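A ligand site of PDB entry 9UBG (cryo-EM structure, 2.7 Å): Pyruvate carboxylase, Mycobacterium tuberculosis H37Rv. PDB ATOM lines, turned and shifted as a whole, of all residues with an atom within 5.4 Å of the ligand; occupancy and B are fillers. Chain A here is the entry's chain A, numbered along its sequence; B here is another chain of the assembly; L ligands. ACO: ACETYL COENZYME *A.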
ATOM      1  N   ARG A 362     -17.859  25.536 -16.031  1.00  0.00           N
ATOM      2  CA  ARG A 362     -18.586  26.015 -14.870  1.00  0.00           C
ATOM      3  C   ARG A 362     -18.761  24.856 -13.911  1.00  0.00           C
ATOM      4  O   ARG A 362     -19.365  23.835 -14.273  1.00  0.00           O
ATOM      5  CB  ARG A 362     -19.943  26.621 -15.255  1.00  0.00           C
ATOM      6  CG  ARG A 362     -19.843  27.996 -15.897  1.00  0.00           C
ATOM      7  CD  ARG A 362     -21.161  28.752 -15.770  1.00  0.00           C
ATOM      8  NE  ARG A 362     -22.304  27.956 -16.196  1.00  0.00           N
ATOM      9  CZ  ARG A 362     -22.904  28.092 -17.377  1.00  0.00           C
ATOM     10  NH1 ARG A 362     -22.497  28.981 -18.258  1.00  0.00           N
ATOM     11  NH2 ARG A 362     -23.943  27.313 -17.656  1.00  0.00           N
ATOM     12  N   ARG A 408     -28.607  17.163  -8.727  1.00  0.00           N
ATOM     13  CA  ARG A 408     -28.461  18.620  -8.812  1.00  0.00           C
ATOM     14  C   ARG A 408     -27.036  19.004  -9.196  1.00  0.00           C
ATOM     15  O   ARG A 408     -26.826  19.890 -10.036  1.00  0.00           O
ATOM     16  CB  ARG A 408     -28.850  19.269  -7.482  1.00  0.00           C
ATOM     17  CG  ARG A 408     -29.112  20.767  -7.569  1.00  0.00           C
ATOM     18  CD  ARG A 408     -27.868  21.572  -7.226  1.00  0.00           C
ATOM     19  NE  ARG A 408     -27.341  21.241  -5.912  1.00  0.00           N
ATOM     20  CZ  ARG A 408     -26.119  21.558  -5.501  1.00  0.00           C
ATOM     21  NH1 ARG A 408     -25.269  22.205  -6.275  1.00  0.00           N
ATOM     22  NH2 ARG A 408     -25.738  21.201  -4.280  1.00  0.00           N
ATOM     23  N   ALA A 411     -26.440  18.314 -12.841  1.00  0.00           N
ATOM     24  CA  ALA A 411     -27.161  19.232 -13.697  1.00  0.00           C
ATOM     25  C   ALA A 411     -26.468  20.597 -13.751  1.00  0.00           C
ATOM     26  O   ALA A 411     -26.339  21.196 -14.833  1.00  0.00           O
ATOM     27  CB  ALA A 411     -28.603  19.383 -13.214  1.00  0.00           C
ATOM     28  N   GLU A 412     -26.032  21.107 -12.600  1.00  0.00           N
ATOM     29  CA  GLU A 412     -25.400  22.423 -12.557  1.00  0.00           C
ATOM     30  C   GLU A 412     -24.078  22.469 -13.314  1.00  0.00           C
ATOM     31  O   GLU A 412     -23.712  23.506 -13.874  1.00  0.00           O
ATOM     32  CB  GLU A 412     -25.202  22.865 -11.110  1.00  0.00           C
ATOM     33  CG  GLU A 412     -24.590  24.247 -10.981  1.00  0.00           C
ATOM     34  CD  GLU A 412     -24.413  24.685  -9.543  1.00  0.00           C
ATOM     35  OE1 GLU A 412     -24.531  23.837  -8.634  1.00  0.00           O
ATOM     36  OE2 GLU A 412     -24.149  25.887  -9.305  1.00  0.00           O
ATOM     37  N   ARG A 414     -21.200  22.387 -16.022  1.00  0.00           N
ATOM     38  CA  ARG A 414     -21.236  22.770 -17.429  1.00  0.00           C
ATOM     39  C   ARG A 414     -19.837  22.657 -18.027  1.00  0.00           C
ATOM     40  O   ARG A 414     -18.897  23.310 -17.554  1.00  0.00           O
ATOM     41  CB  ARG A 414     -21.772  24.197 -17.610  1.00  0.00           C
ATOM     42  CG  ARG A 414     -22.485  24.408 -18.930  1.00  0.00           C
ATOM     43  CD  ARG A 414     -23.833  23.710 -18.952  1.00  0.00           C
ATOM     44  NE  ARG A 414     -24.833  24.421 -18.156  1.00  0.00           N
ATOM     45  CZ  ARG A 414     -25.903  23.848 -17.622  1.00  0.00           C
ATOM     46  NH1 ARG A 414     -26.152  22.560 -17.775  1.00  0.00           N
ATOM     47  NH2 ARG A 414     -26.742  24.596 -16.909  1.00  0.00           N
ATOM     48  N   ARG A 416     -18.078  22.777 -21.916  1.00  0.00           N
ATOM     49  CA  ARG A 416     -18.265  23.052 -23.335  1.00  0.00           C
ATOM     50  C   ARG A 416     -16.911  23.062 -24.030  1.00  0.00           C
ATOM     51  O   ARG A 416     -15.965  23.699 -23.553  1.00  0.00           O
ATOM     52  CB  ARG A 416     -18.970  24.392 -23.570  1.00  0.00           C
ATOM     53  CG  ARG A 416     -20.294  24.519 -22.849  1.00  0.00           C
ATOM     54  CD  ARG A 416     -21.439  24.086 -23.736  1.00  0.00           C
ATOM     55  NE  ARG A 416     -22.727  24.357 -23.120  1.00  0.00           N
ATOM     56  CZ  ARG A 416     -23.737  23.504 -23.088  1.00  0.00           C
ATOM     57  NH1 ARG A 416     -23.619  22.288 -23.601  1.00  0.00           N
ATOM     58  NH2 ARG A 416     -24.879  23.858 -22.528  1.00  0.00           N
ATOM     59  N   ALA A 455     -28.167  15.427 -26.168  1.00  0.00           N
ATOM     60  CA  ALA A 455     -26.939  15.769 -25.463  1.00  0.00           C
ATOM     61  C   ALA A 455     -27.055  17.103 -24.734  1.00  0.00           C
ATOM     62  O   ALA A 455     -27.036  17.142 -23.503  1.00  0.00           O
ATOM     63  CB  ALA A 455     -25.764  15.818 -26.444  1.00  0.00           C
ATOM     64  N   SER A 456     -27.154  18.197 -25.481  1.00  0.00           N
ATOM     65  CA  SER A 456     -27.319  19.504 -24.862  1.00  0.00           C
ATOM     66  C   SER A 456     -28.280  20.456 -25.566  1.00  0.00           C
ATOM     67  O   SER A 456     -28.855  21.309 -24.891  1.00  0.00           O
ATOM     68  CB  SER A 456     -25.958  20.183 -24.711  1.00  0.00           C
ATOM     69  OG  SER A 456     -25.820  21.559 -24.977  1.00  0.00           O
ATOM     70  N   ALA A 457     -28.496  20.326 -26.877  1.00  0.00           N
ATOM     71  CA  ALA A 457     -29.272  21.298 -27.642  1.00  0.00           C
ATOM     72  C   ALA A 457     -28.793  22.721 -27.357  1.00  0.00           C
ATOM     73  O   ALA A 457     -29.563  23.620 -27.044  1.00  0.00           O
ATOM     74  CB  ALA A 457     -30.772  21.153 -27.374  1.00  0.00           C
ATOM     75  N   ASP A 458     -27.476  22.904 -27.488  1.00  0.00           N
ATOM     76  CA  ASP A 458     -26.817  24.117 -27.042  1.00  0.00           C
ATOM     77  C   ASP A 458     -27.007  25.216 -28.093  1.00  0.00           C
ATOM     78  O   ASP A 458     -26.511  25.093 -29.212  1.00  0.00           O
ATOM     79  CB  ASP A 458     -25.332  23.879 -26.781  1.00  0.00           C
ATOM     80  CG  ASP A 458     -24.648  23.010 -27.854  1.00  0.00           C
ATOM     81  OD1 ASP A 458     -25.276  22.124 -28.472  1.00  0.00           O
ATOM     82  OD2 ASP A 458     -23.438  23.210 -28.060  1.00  0.00           O
ATOM     83  N   ARG A 459     -27.706  26.278 -27.709  1.00  0.00           N
ATOM     84  CA  ARG A 459     -28.026  27.359 -28.642  1.00  0.00           C
ATOM     85  C   ARG A 459     -26.999  28.468 -28.586  1.00  0.00           C
ATOM     86  O   ARG A 459     -26.706  29.088 -29.622  1.00  0.00           O
ATOM     87  CB  ARG A 459     -29.410  27.897 -28.283  1.00  0.00           C
ATOM     88  CG  ARG A 459     -30.439  26.787 -28.215  1.00  0.00           C
ATOM     89  CD  ARG A 459     -31.869  27.263 -28.037  1.00  0.00           C
ATOM     90  NE  ARG A 459     -32.303  27.161 -26.646  1.00  0.00           N
ATOM     91  CZ  ARG A 459     -33.415  27.702 -26.164  1.00  0.00           C
ATOM     92  NH1 ARG A 459     -34.229  28.400 -26.936  1.00  0.00           N
ATOM     93  NH2 ARG A 459     -33.710  27.534 -24.880  1.00  0.00           N
ATOM     94  N   GLY A 460     -26.430  28.735 -27.412  1.00  0.00           N
ATOM     95  CA  GLY A 460     -25.447  29.801 -27.287  1.00  0.00           C
ATOM     96  C   GLY A 460     -24.201  29.545 -28.108  1.00  0.00           C
ATOM     97  O   GLY A 460     -23.674  30.454 -28.759  1.00  0.00           O
ATOM     98  N   THR A 461     -23.721  28.304 -28.112  1.00  0.00           N
ATOM     99  CA  THR A 461     -22.509  27.965 -28.862  1.00  0.00           C
ATOM    100  C   THR A 461     -22.729  28.094 -30.364  1.00  0.00           C
ATOM    101  O   THR A 461     -21.834  28.542 -31.091  1.00  0.00           O
ATOM    102  CB  THR A 461     -22.042  26.558 -28.505  1.00  0.00           C
ATOM    103  OG1 THR A 461     -22.699  25.604 -29.353  1.00  0.00           O
ATOM    104  CG2 THR A 461     -22.364  26.240 -27.055  1.00  0.00           C
ATOM    105  N   LEU A1002     -34.047  34.887 -26.429  1.00  0.00           N
ATOM    106  CA  LEU A1002     -34.325  33.488 -26.751  1.00  0.00           C
ATOM    107  C   LEU A1002     -35.737  33.080 -26.353  1.00  0.00           C
ATOM    108  O   LEU A1002     -36.501  32.576 -27.191  1.00  0.00           O
ATOM    109  CB  LEU A1002     -33.303  32.569 -26.053  1.00  0.00           C
ATOM    110  CG  LEU A1002     -32.286  31.887 -26.961  1.00  0.00           C
ATOM    111  CD1 LEU A1002     -31.357  32.898 -27.604  1.00  0.00           C
ATOM    112  CD2 LEU A1002     -31.488  30.843 -26.186  1.00  0.00           C
ATOM    113  N   GLY A1005     -38.020  35.750 -20.552  1.00  0.00           N
ATOM    114  CA  GLY A1005     -37.116  35.698 -19.422  1.00  0.00           C
ATOM    115  C   GLY A1005     -35.783  35.053 -19.708  1.00  0.00           C
ATOM    116  O   GLY A1005     -34.950  34.974 -18.806  1.00  0.00           O
ATOM    117  N   VAL A1006     -35.559  34.572 -20.934  1.00  0.00           N
ATOM    118  CA  VAL A1006     -34.315  33.921 -21.317  1.00  0.00           C
ATOM    119  C   VAL A1006     -33.657  34.806 -22.375  1.00  0.00           C
ATOM    120  O   VAL A1006     -34.034  34.759 -23.549  1.00  0.00           O
ATOM    121  CB  VAL A1006     -34.544  32.500 -21.825  1.00  0.00           C
ATOM    122  CG1 VAL A1006     -33.233  31.873 -22.256  1.00  0.00           C
ATOM    123  CG2 VAL A1006     -35.214  31.658 -20.755  1.00  0.00           C
ATOM    124  N   GLU A1007     -32.665  35.585 -21.950  1.00  0.00           N
ATOM    125  CA  GLU A1007     -31.956  36.516 -22.823  1.00  0.00           C
ATOM    126  C   GLU A1007     -30.455  36.267 -22.725  1.00  0.00           C
ATOM    127  O   GLU A1007     -29.948  35.820 -21.695  1.00  0.00           O
ATOM    128  CB  GLU A1007     -32.261  37.972 -22.441  1.00  0.00           C
ATOM    129  CG  GLU A1007     -33.655  38.441 -22.818  1.00  0.00           C
ATOM    130  CD  GLU A1007     -34.035  39.739 -22.129  1.00  0.00           C
ATOM    131  OE1 GLU A1007     -33.164  40.331 -21.470  1.00  0.00           O
ATOM    132  OE2 GLU A1007     -35.204  40.155 -22.262  1.00  0.00           O
ATOM    133  N   LEU A1008     -29.752  36.567 -23.817  1.00  0.00           N
ATOM    134  CA  LEU A1008     -28.314  36.330 -23.934  1.00  0.00           C
ATOM    135  C   LEU A1008     -27.600  37.649 -24.223  1.00  0.00           C
ATOM    136  O   LEU A1008     -28.045  38.432 -25.060  1.00  0.00           O
ATOM    137  CB  LEU A1008     -28.007  35.319 -25.032  1.00  0.00           C
ATOM    138  CG  LEU A1008     -27.792  33.856 -24.638  1.00  0.00           C
ATOM    139  CD1 LEU A1008     -28.954  33.328 -23.820  1.00  0.00           C
ATOM    140  CD2 LEU A1008     -27.567  33.001 -25.874  1.00  0.00           C
ATOM    141  N   LEU A1030     -19.741  35.900 -23.396  1.00  0.00           N
ATOM    142  CA  LEU A1030     -21.120  35.426 -23.330  1.00  0.00           C
ATOM    143  C   LEU A1030     -21.536  35.368 -21.865  1.00  0.00           C
ATOM    144  O   LEU A1030     -20.921  34.650 -21.064  1.00  0.00           O
ATOM    145  CB  LEU A1030     -21.259  34.050 -23.988  1.00  0.00           C
ATOM    146  CG  LEU A1030     -22.692  33.567 -24.159  1.00  0.00           C
ATOM    147  CD1 LEU A1030     -23.487  34.075 -25.362  1.00  0.00           C
ATOM    148  CD2 LEU A1030     -22.822  32.047 -24.023  1.00  0.00           C
ATOM    149  N   ASN A1031     -22.551  36.158 -21.510  1.00  0.00           N
ATOM    150  CA  ASN A1031     -23.057  36.252 -20.139  1.00  0.00           C
ATOM    151  C   ASN A1031     -21.932  36.587 -19.162  1.00  0.00           C
ATOM    152  O   ASN A1031     -21.896  36.099 -18.023  1.00  0.00           O
ATOM    153  CB  ASN A1031     -23.763  34.956 -19.744  1.00  0.00           C
ATOM    154  CG  ASN A1031     -25.159  34.860 -20.332  1.00  0.00           C
ATOM    155  OD1 ASN A1031     -25.835  35.867 -20.502  1.00  0.00           O
ATOM    156  ND2 ASN A1031     -25.578  33.643 -20.659  1.00  0.00           N
ATOM    157  N   GLN A1033     -18.745  35.819 -19.505  1.00  0.00           N
ATOM    158  CA  GLN A1033     -17.738  34.760 -19.442  1.00  0.00           C
ATOM    159  C   GLN A1033     -16.969  34.713 -20.753  1.00  0.00           C
ATOM    160  O   GLN A1033     -17.550  34.874 -21.835  1.00  0.00           O
ATOM    161  CB  GLN A1033     -18.378  33.405 -19.151  1.00  0.00           C
ATOM    162  CG  GLN A1033     -19.272  33.400 -17.918  1.00  0.00           C
ATOM    163  CD  GLN A1033     -19.962  32.075 -17.712  1.00  0.00           C
ATOM    164  OE1 GLN A1033     -20.639  31.857 -16.706  1.00  0.00           O
ATOM    165  NE2 GLN A1033     -19.821  31.163 -18.677  1.00  0.00           N
ATOM    166  N   ARG A1035     -15.006  33.228 -23.921  1.00  0.00           N
ATOM    167  CA  ARG A1035     -15.178  32.065 -24.788  1.00  0.00           C
ATOM    168  C   ARG A1035     -14.270  32.172 -26.011  1.00  0.00           C
ATOM    169  O   ARG A1035     -14.367  33.135 -26.782  1.00  0.00           O
ATOM    170  CB  ARG A1035     -16.632  31.930 -25.223  1.00  0.00           C
ATOM    171  CG  ARG A1035     -17.610  31.593 -24.114  1.00  0.00           C
ATOM    172  CD  ARG A1035     -18.057  30.148 -24.202  1.00  0.00           C
ATOM    173  NE  ARG A1035     -19.339  29.931 -23.557  1.00  0.00           N
ATOM    174  CZ  ARG A1035     -20.289  29.125 -24.022  1.00  0.00           C
ATOM    175  NH1 ARG A1035     -20.125  28.442 -25.141  1.00  0.00           N
ATOM    176  NH2 ARG A1035     -21.428  29.000 -23.342  1.00  0.00           N
ATOM    177  N   PHE B  18     -31.764  28.668  -5.031  1.00  0.00           N
ATOM    178  CA  PHE B  18     -32.061  28.002  -6.300  1.00  0.00           C
ATOM    179  C   PHE B  18     -31.727  26.524  -6.236  1.00  0.00           C
ATOM    180  O   PHE B  18     -32.503  25.687  -6.724  1.00  0.00           O
ATOM    181  CB  PHE B  18     -31.288  28.669  -7.437  1.00  0.00           C
ATOM    182  CG  PHE B  18     -31.724  30.077  -7.731  1.00  0.00           C
ATOM    183  CD1 PHE B  18     -33.025  30.482  -7.494  1.00  0.00           C
ATOM    184  CD2 PHE B  18     -30.835  30.998  -8.273  1.00  0.00           C
ATOM    185  CE1 PHE B  18     -33.432  31.774  -7.768  1.00  0.00           C
ATOM    186  CE2 PHE B  18     -31.231  32.285  -8.559  1.00  0.00           C
ATOM    187  CZ  PHE B  18     -32.528  32.677  -8.304  1.00  0.00           C
ATOM    188  N   ARG B  19     -30.582  26.178  -5.640  1.00  0.00           N
ATOM    189  CA  ARG B  19     -30.212  24.769  -5.507  1.00  0.00           C
ATOM    190  C   ARG B  19     -31.211  24.018  -4.629  1.00  0.00           C
ATOM    191  O   ARG B  19     -31.625  22.903  -4.961  1.00  0.00           O
ATOM    192  CB  ARG B  19     -28.805  24.650  -4.931  1.00  0.00           C
ATOM    193  CG  ARG B  19     -27.699  25.121  -5.869  1.00  0.00           C
ATOM    194  CD  ARG B  19     -26.382  25.265  -5.126  1.00  0.00           C
ATOM    195  NE  ARG B  19     -25.272  25.572  -6.022  1.00  0.00           N
ATOM    196  CZ  ARG B  19     -24.194  26.261  -5.677  1.00  0.00           C
ATOM    197  NH1 ARG B  19     -24.044  26.731  -4.452  1.00  0.00           N
ATOM    198  NH2 ARG B  19     -23.250  26.485  -6.585  1.00  0.00           N
ATOM    199  N   TYR B  22     -34.400  23.497  -6.625  1.00  0.00           N
ATOM    200  CA  TYR B  22     -34.253  22.456  -7.636  1.00  0.00           C
ATOM    201  C   TYR B  22     -34.237  21.075  -7.008  1.00  0.00           C
ATOM    202  O   TYR B  22     -34.743  20.115  -7.595  1.00  0.00           O
ATOM    203  CB  TYR B  22     -32.979  22.684  -8.451  1.00  0.00           C
ATOM    204  CG  TYR B  22     -32.824  21.728  -9.617  1.00  0.00           C
ATOM    205  CD1 TYR B  22     -33.415  21.986 -10.851  1.00  0.00           C
ATOM    206  CD2 TYR B  22     -32.091  20.551  -9.477  1.00  0.00           C
ATOM    207  CE1 TYR B  22     -33.271  21.111 -11.904  1.00  0.00           C
ATOM    208  CE2 TYR B  22     -31.948  19.667 -10.536  1.00  0.00           C
ATOM    209  CZ  TYR B  22     -32.547  19.955 -11.741  1.00  0.00           C
ATOM    210  OH  TYR B  22     -32.403  19.080 -12.794  1.00  0.00           O
ATOM    211  N   ARG B  42     -28.249  35.561 -12.257  1.00  0.00           N
ATOM    212  CA  ARG B  42     -29.181  35.776 -13.352  1.00  0.00           C
ATOM    213  C   ARG B  42     -29.253  34.561 -14.268  1.00  0.00           C
ATOM    214  O   ARG B  42     -30.336  34.183 -14.721  1.00  0.00           O
ATOM    215  CB  ARG B  42     -28.781  37.025 -14.147  1.00  0.00           C
ATOM    216  CG  ARG B  42     -29.659  37.277 -15.373  1.00  0.00           C
ATOM    217  CD  ARG B  42     -29.288  38.574 -16.058  1.00  0.00           C
ATOM    218  NE  ARG B  42     -28.279  38.387 -17.091  1.00  0.00           N
ATOM    219  CZ  ARG B  42     -28.520  37.937 -18.310  1.00  0.00           C
ATOM    220  NH1 ARG B  42     -29.753  37.599 -18.689  1.00  0.00           N
ATOM    221  NH2 ARG B  42     -27.519  37.802 -19.173  1.00  0.00           N
ATOM    222  N   LEU B  43     -28.116  33.927 -14.552  1.00  0.00           N
ATOM    223  CA  LEU B  43     -28.088  32.808 -15.482  1.00  0.00           C
ATOM    224  C   LEU B  43     -28.274  31.458 -14.792  1.00  0.00           C
ATOM    225  O   LEU B  43     -28.268  30.424 -15.473  1.00  0.00           O
ATOM    226  CB  LEU B  43     -26.783  32.799 -16.281  1.00  0.00           C
ATOM    227  CG  LEU B  43     -25.452  32.882 -15.524  1.00  0.00           C
ATOM    228  CD1 LEU B  43     -24.809  31.513 -15.393  1.00  0.00           C
ATOM    229  CD2 LEU B  43     -24.504  33.850 -16.213  1.00  0.00           C
ATOM    230  N   LYS B  44     -28.442  31.446 -13.472  1.00  0.00           N
ATOM    231  CA  LYS B  44     -28.670  30.214 -12.731  1.00  0.00           C
ATOM    232  C   LYS B  44     -30.149  29.914 -12.509  1.00  0.00           C
ATOM    233  O   LYS B  44     -30.468  28.856 -11.947  1.00  0.00           O
ATOM    234  CB  LYS B  44     -27.947  30.265 -11.383  1.00  0.00           C
ATOM    235  CG  LYS B  44     -26.438  30.433 -11.494  1.00  0.00           C
ATOM    236  CD  LYS B  44     -25.709  29.163 -11.117  1.00  0.00           C
ATOM    237  CE  LYS B  44     -24.388  29.046 -11.870  1.00  0.00           C
ATOM    238  NZ  LYS B  44     -23.353  28.326 -11.073  1.00  0.00           N
ATOM    239  N   ALA B  45     -31.042  30.800 -12.922  1.00  0.00           N
ATOM    240  CA  ALA B  45     -32.471  30.648 -12.710  1.00  0.00           C
ATOM    241  C   ALA B  45     -33.171  30.307 -14.017  1.00  0.00           C
ATOM    242  O   ALA B  45     -32.636  30.520 -15.113  1.00  0.00           O
ATOM    243  CB  ALA B  45     -33.073  31.921 -12.103  1.00  0.00           C
ATOM    244  N   ASP B  46     -34.381  29.766 -13.886  1.00  0.00           N
ATOM    245  CA  ASP B  46     -35.168  29.419 -15.065  1.00  0.00           C
ATOM    246  C   ASP B  46     -35.616  30.654 -15.827  1.00  0.00           C
ATOM    247  O   ASP B  46     -35.550  30.695 -17.064  1.00  0.00           O
ATOM    248  CB  ASP B  46     -36.380  28.566 -14.666  1.00  0.00           C
ATOM    249  CG  ASP B  46     -35.994  27.244 -14.031  1.00  0.00           C
ATOM    250  OD1 ASP B  46     -34.820  27.072 -13.635  1.00  0.00           O
ATOM    251  OD2 ASP B  46     -36.867  26.365 -13.919  1.00  0.00           O
ATOM    252  N   GLU B  47     -36.068  31.686 -15.115  1.00  0.00           N
ATOM    253  CA  GLU B  47     -36.508  32.930 -15.733  1.00  0.00           C
ATOM    254  C   GLU B  47     -35.937  34.111 -14.964  1.00  0.00           C
ATOM    255  O   GLU B  47     -35.798  34.049 -13.733  1.00  0.00           O
ATOM    256  CB  GLU B  47     -38.040  33.018 -15.772  1.00  0.00           C
ATOM    257  CG  GLU B  47     -38.703  31.996 -16.680  1.00  0.00           C
ATOM    258  CD  GLU B  47     -40.140  31.700 -16.279  1.00  0.00           C
ATOM    259  OE1 GLU B  47     -40.918  32.655 -16.131  1.00  0.00           O
ATOM    260  OE2 GLU B  47     -40.472  30.510 -16.120  1.00  0.00           O
ATOM    261  N   SER B  48     -35.618  35.180 -15.682  1.00  0.00           N
ATOM    262  CA  SER B  48     -35.070  36.390 -15.090  1.00  0.00           C
ATOM    263  C   SER B  48     -35.790  37.612 -15.644  1.00  0.00           C
ATOM    264  O   SER B  48     -36.202  37.638 -16.808  1.00  0.00           O
ATOM    265  CB  SER B  48     -33.568  36.514 -15.345  1.00  0.00           C
ATOM    266  OG  SER B  48     -32.943  35.245 -15.317  1.00  0.00           O
HETATM  267  N1A ACO L   1     -30.746  33.772 -18.371  1.00  0.00           N
HETATM  268  C2A ACO L   1     -29.673  33.809 -19.158  1.00  0.00           C
HETATM  269  N3A ACO L   1     -29.052  32.830 -19.801  1.00  0.00           N
HETATM  270  C4A ACO L   1     -29.659  31.651 -19.556  1.00  0.00           C
HETATM  271  C5A ACO L   1     -30.766  31.445 -18.767  1.00  0.00           C
HETATM  272  C6A ACO L   1     -31.335  32.570 -18.148  1.00  0.00           C
HETATM  273  N6A ACO L   1     -32.409  32.525 -17.366  1.00  0.00           N
HETATM  274  N7A ACO L   1     -31.107  30.103 -18.775  1.00  0.00           N
HETATM  275  C8A ACO L   1     -30.214  29.532 -19.540  1.00  0.00           C
HETATM  276  N9A ACO L   1     -29.316  30.425 -20.060  1.00  0.00           N
HETATM  277  C1B ACO L   1     -28.181  30.120 -20.914  1.00  0.00           C
HETATM  278  C2B ACO L   1     -27.548  28.795 -20.495  1.00  0.00           C
HETATM  279  O2B ACO L   1     -26.508  29.013 -19.563  1.00  0.00           O
HETATM  280  C3B ACO L   1     -27.039  28.244 -21.830  1.00  0.00           C
HETATM  281  O3B ACO L   1     -25.759  28.800 -22.152  1.00  0.00           O
HETATM  282  P3B ACO L   1     -24.559  27.762 -21.857  1.00  0.00           P
HETATM  283  O7A ACO L   1     -25.101  26.644 -21.013  1.00  0.00           O
HETATM  284  O8A ACO L   1     -23.512  28.563 -21.124  1.00  0.00           O
HETATM  285  O9A ACO L   1     -24.080  27.294 -23.199  1.00  0.00           O
HETATM  286  C4B ACO L   1     -28.117  28.718 -22.793  1.00  0.00           C
HETATM  287  O4B ACO L   1     -28.610  29.966 -22.240  1.00  0.00           O
HETATM  288  C5B ACO L   1     -29.280  27.778 -22.959  1.00  0.00           C
HETATM  289  O5B ACO L   1     -28.854  26.561 -23.615  1.00  0.00           O
HETATM  290  P1A ACO L   1     -29.922  25.370 -23.564  1.00  0.00           P
HETATM  291  O1A ACO L   1     -30.399  25.073 -24.939  1.00  0.00           O
HETATM  292  O2A ACO L   1     -30.951  25.683 -22.531  1.00  0.00           O
HETATM  293  O3A ACO L   1     -29.005  24.152 -23.051  1.00  0.00           O
HETATM  294  P2A ACO L   1     -29.257  22.786 -22.256  1.00  0.00           P
HETATM  295  O4A ACO L   1     -30.537  22.165 -22.714  1.00  0.00           O
HETATM  296  O5A ACO L   1     -28.008  21.982 -22.302  1.00  0.00           O
HETATM  297  O6A ACO L   1     -29.454  23.284 -20.747  1.00  0.00           O
HETATM  298  CBP ACO L   1     -30.703  23.894 -18.770  1.00  0.00           C
HETATM  299  CCP ACO L   1     -30.779  23.271 -20.157  1.00  0.00           C
HETATM  300  CDP ACO L   1     -32.116  24.076 -18.231  1.00  0.00           C
HETATM  301  CEP ACO L   1     -29.948  22.948 -17.845  1.00  0.00           C
HETATM  302  CAP ACO L   1     -29.981  25.251 -18.818  1.00  0.00           C
HETATM  303  OAP ACO L   1     -29.903  25.673 -20.161  1.00  0.00           O
HETATM  304  C9P ACO L   1     -30.625  26.350 -17.992  1.00  0.00           C
HETATM  305  O9P ACO L   1     -31.531  27.021 -18.464  1.00  0.00           O
HETATM  306  N8P ACO L   1     -30.142  26.560 -16.773  1.00  0.00           N
HETATM  307  C7P ACO L   1     -30.833  27.379 -15.786  1.00  0.00           C
HETATM  308  C6P ACO L   1     -31.132  26.604 -14.529  1.00  0.00           C
HETATM  309  C5P ACO L   1     -30.323  25.329 -14.491  1.00  0.00           C
HETATM  310  O5P ACO L   1     -29.096  25.353 -14.521  1.00  0.00           O
HETATM  311  N4P ACO L   1     -30.995  24.176 -14.427  1.00  0.00           N
HETATM  312  C3P ACO L   1     -30.398  22.934 -13.978  1.00  0.00           C
HETATM  313  C2P ACO L   1     -30.429  22.810 -12.473  1.00  0.00           C
HETATM  314  S1P ACO L   1     -29.138  23.822 -11.752  1.00  0.00           S
HETATM  315  C   ACO L   1     -29.337  24.739 -10.278  1.00  0.00           C
HETATM  316  O   ACO L   1     -28.993  25.882 -10.164  1.00  0.00           O
HETATM  317  CH3 ACO L   1     -29.945  23.950  -9.189  1.00  0.00           C
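Merely in contact with the ligand: Glu 1007, Tyr 22 of chain B, Lys 44 of chain B, Asp 46 of chain B, Arg 408, Asn 1031, Arg 42 of chain B, Leu 1008, Arg 19 of chain B, Gly 1005, Ala 411, Phe 18 of chain B and Leu 43 of chain B.
Hydrophobic or aromatic side chains within 4 Å of the ligand: Ala 411, Leu 1008 and Tyr 22 of chain B.
22 residues have an atom within 4 Å of the ligand: Arg 362, Arg 408, Ala 411, Arg 414, Arg 416, Ser 456, Ala 457, Arg 459, Gly 1005, Glu 1007, Leu 1008, Asn 1031, Arg 1035, Phe 18 of chain B, Arg 19 of chain B, Tyr 22 of chain B, Arg 42 of chain B, Leu 43 of chain B, Lys 44 of chain B, Ala 45 of chain B, Asp 46 of chain B and Ser 48 of chain B.
The guanidinium group (NH2) of Arg 42 of chain B is in hydrogen-bond range of the side-chain amide oxygen (OD1) of Asn 1031 (2.9 Å).
The side-chain hydroxyl (OG) of Ser 456 is in hydrogen-bond range of the guanidinium group (NH1) of Arg 416 (2.7 Å).
NZ of Lys 44 of chain B is in salt-bridge range of OE2 of Glu 412, 3.1 Å away.
NH1 of Arg 362 lies close to NE2 of Gln 1033 (3.5 Å).
The backbone carbonyl oxygen of Arg 414 lies within hydrogen-bond range of the backbone NH of Arg 362 (2.9 Å).
The side-chain carboxylate (OE1) of Glu 412 lies within salt-bridge range of the guanidinium group (NH1) of Arg 408 (3.0 Å).
The guanidinium group of Arg 19 of chain B lies within salt-bridge range of the side-chain carboxylate of Glu 412, 2.9 Å away.
The side-chain hydroxyl (OG) of Ser 48 of chain B lies within hydrogen-bond range of the backbone carbonyl oxygen (O) of Arg 42 of chain B (2.9 Å).
An oxygen (O5A) of the ligand is in hydrogen-bond range of the side-chain hydroxyl (OG) of Ser 456 (3.5 Å).
An oxygen (O8A) of the ligand lies within salt-bridge range of the guanidinium group (NH2) of Arg 1035, 3.1 Å away.
The guanidinium group (NE) of Arg 414 lies within salt-bridge range of an oxygen (O7A) of the ligand (3.6 Å).
N6A of the ligand sits at hydrogen-bond distance from OG of Ser 48 of chain B (3.4 Å).
The guanidinium group (NE) of Arg 459 lies within salt-bridge range of an oxygen (O1A) of the ligand, 3.3 Å away.
The backbone carbonyl oxygen of Ala 45 of chain B sits at hydrogen-bond distance from a nitrogen (N6A) of the ligand.
An oxygen (O5A) of the ligand sits close to the backbone carbonyl oxygen (O) of Ser 456 (2.8 Å).
O of Ala 457 lies close to O1A of the ligand.
The guanidinium group of Arg 362 is in salt-bridge range of an oxygen (O8A) of the ligand.
NH2 of Arg 416 lies within salt-bridge range of O7A of the ligand (3.2 Å).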
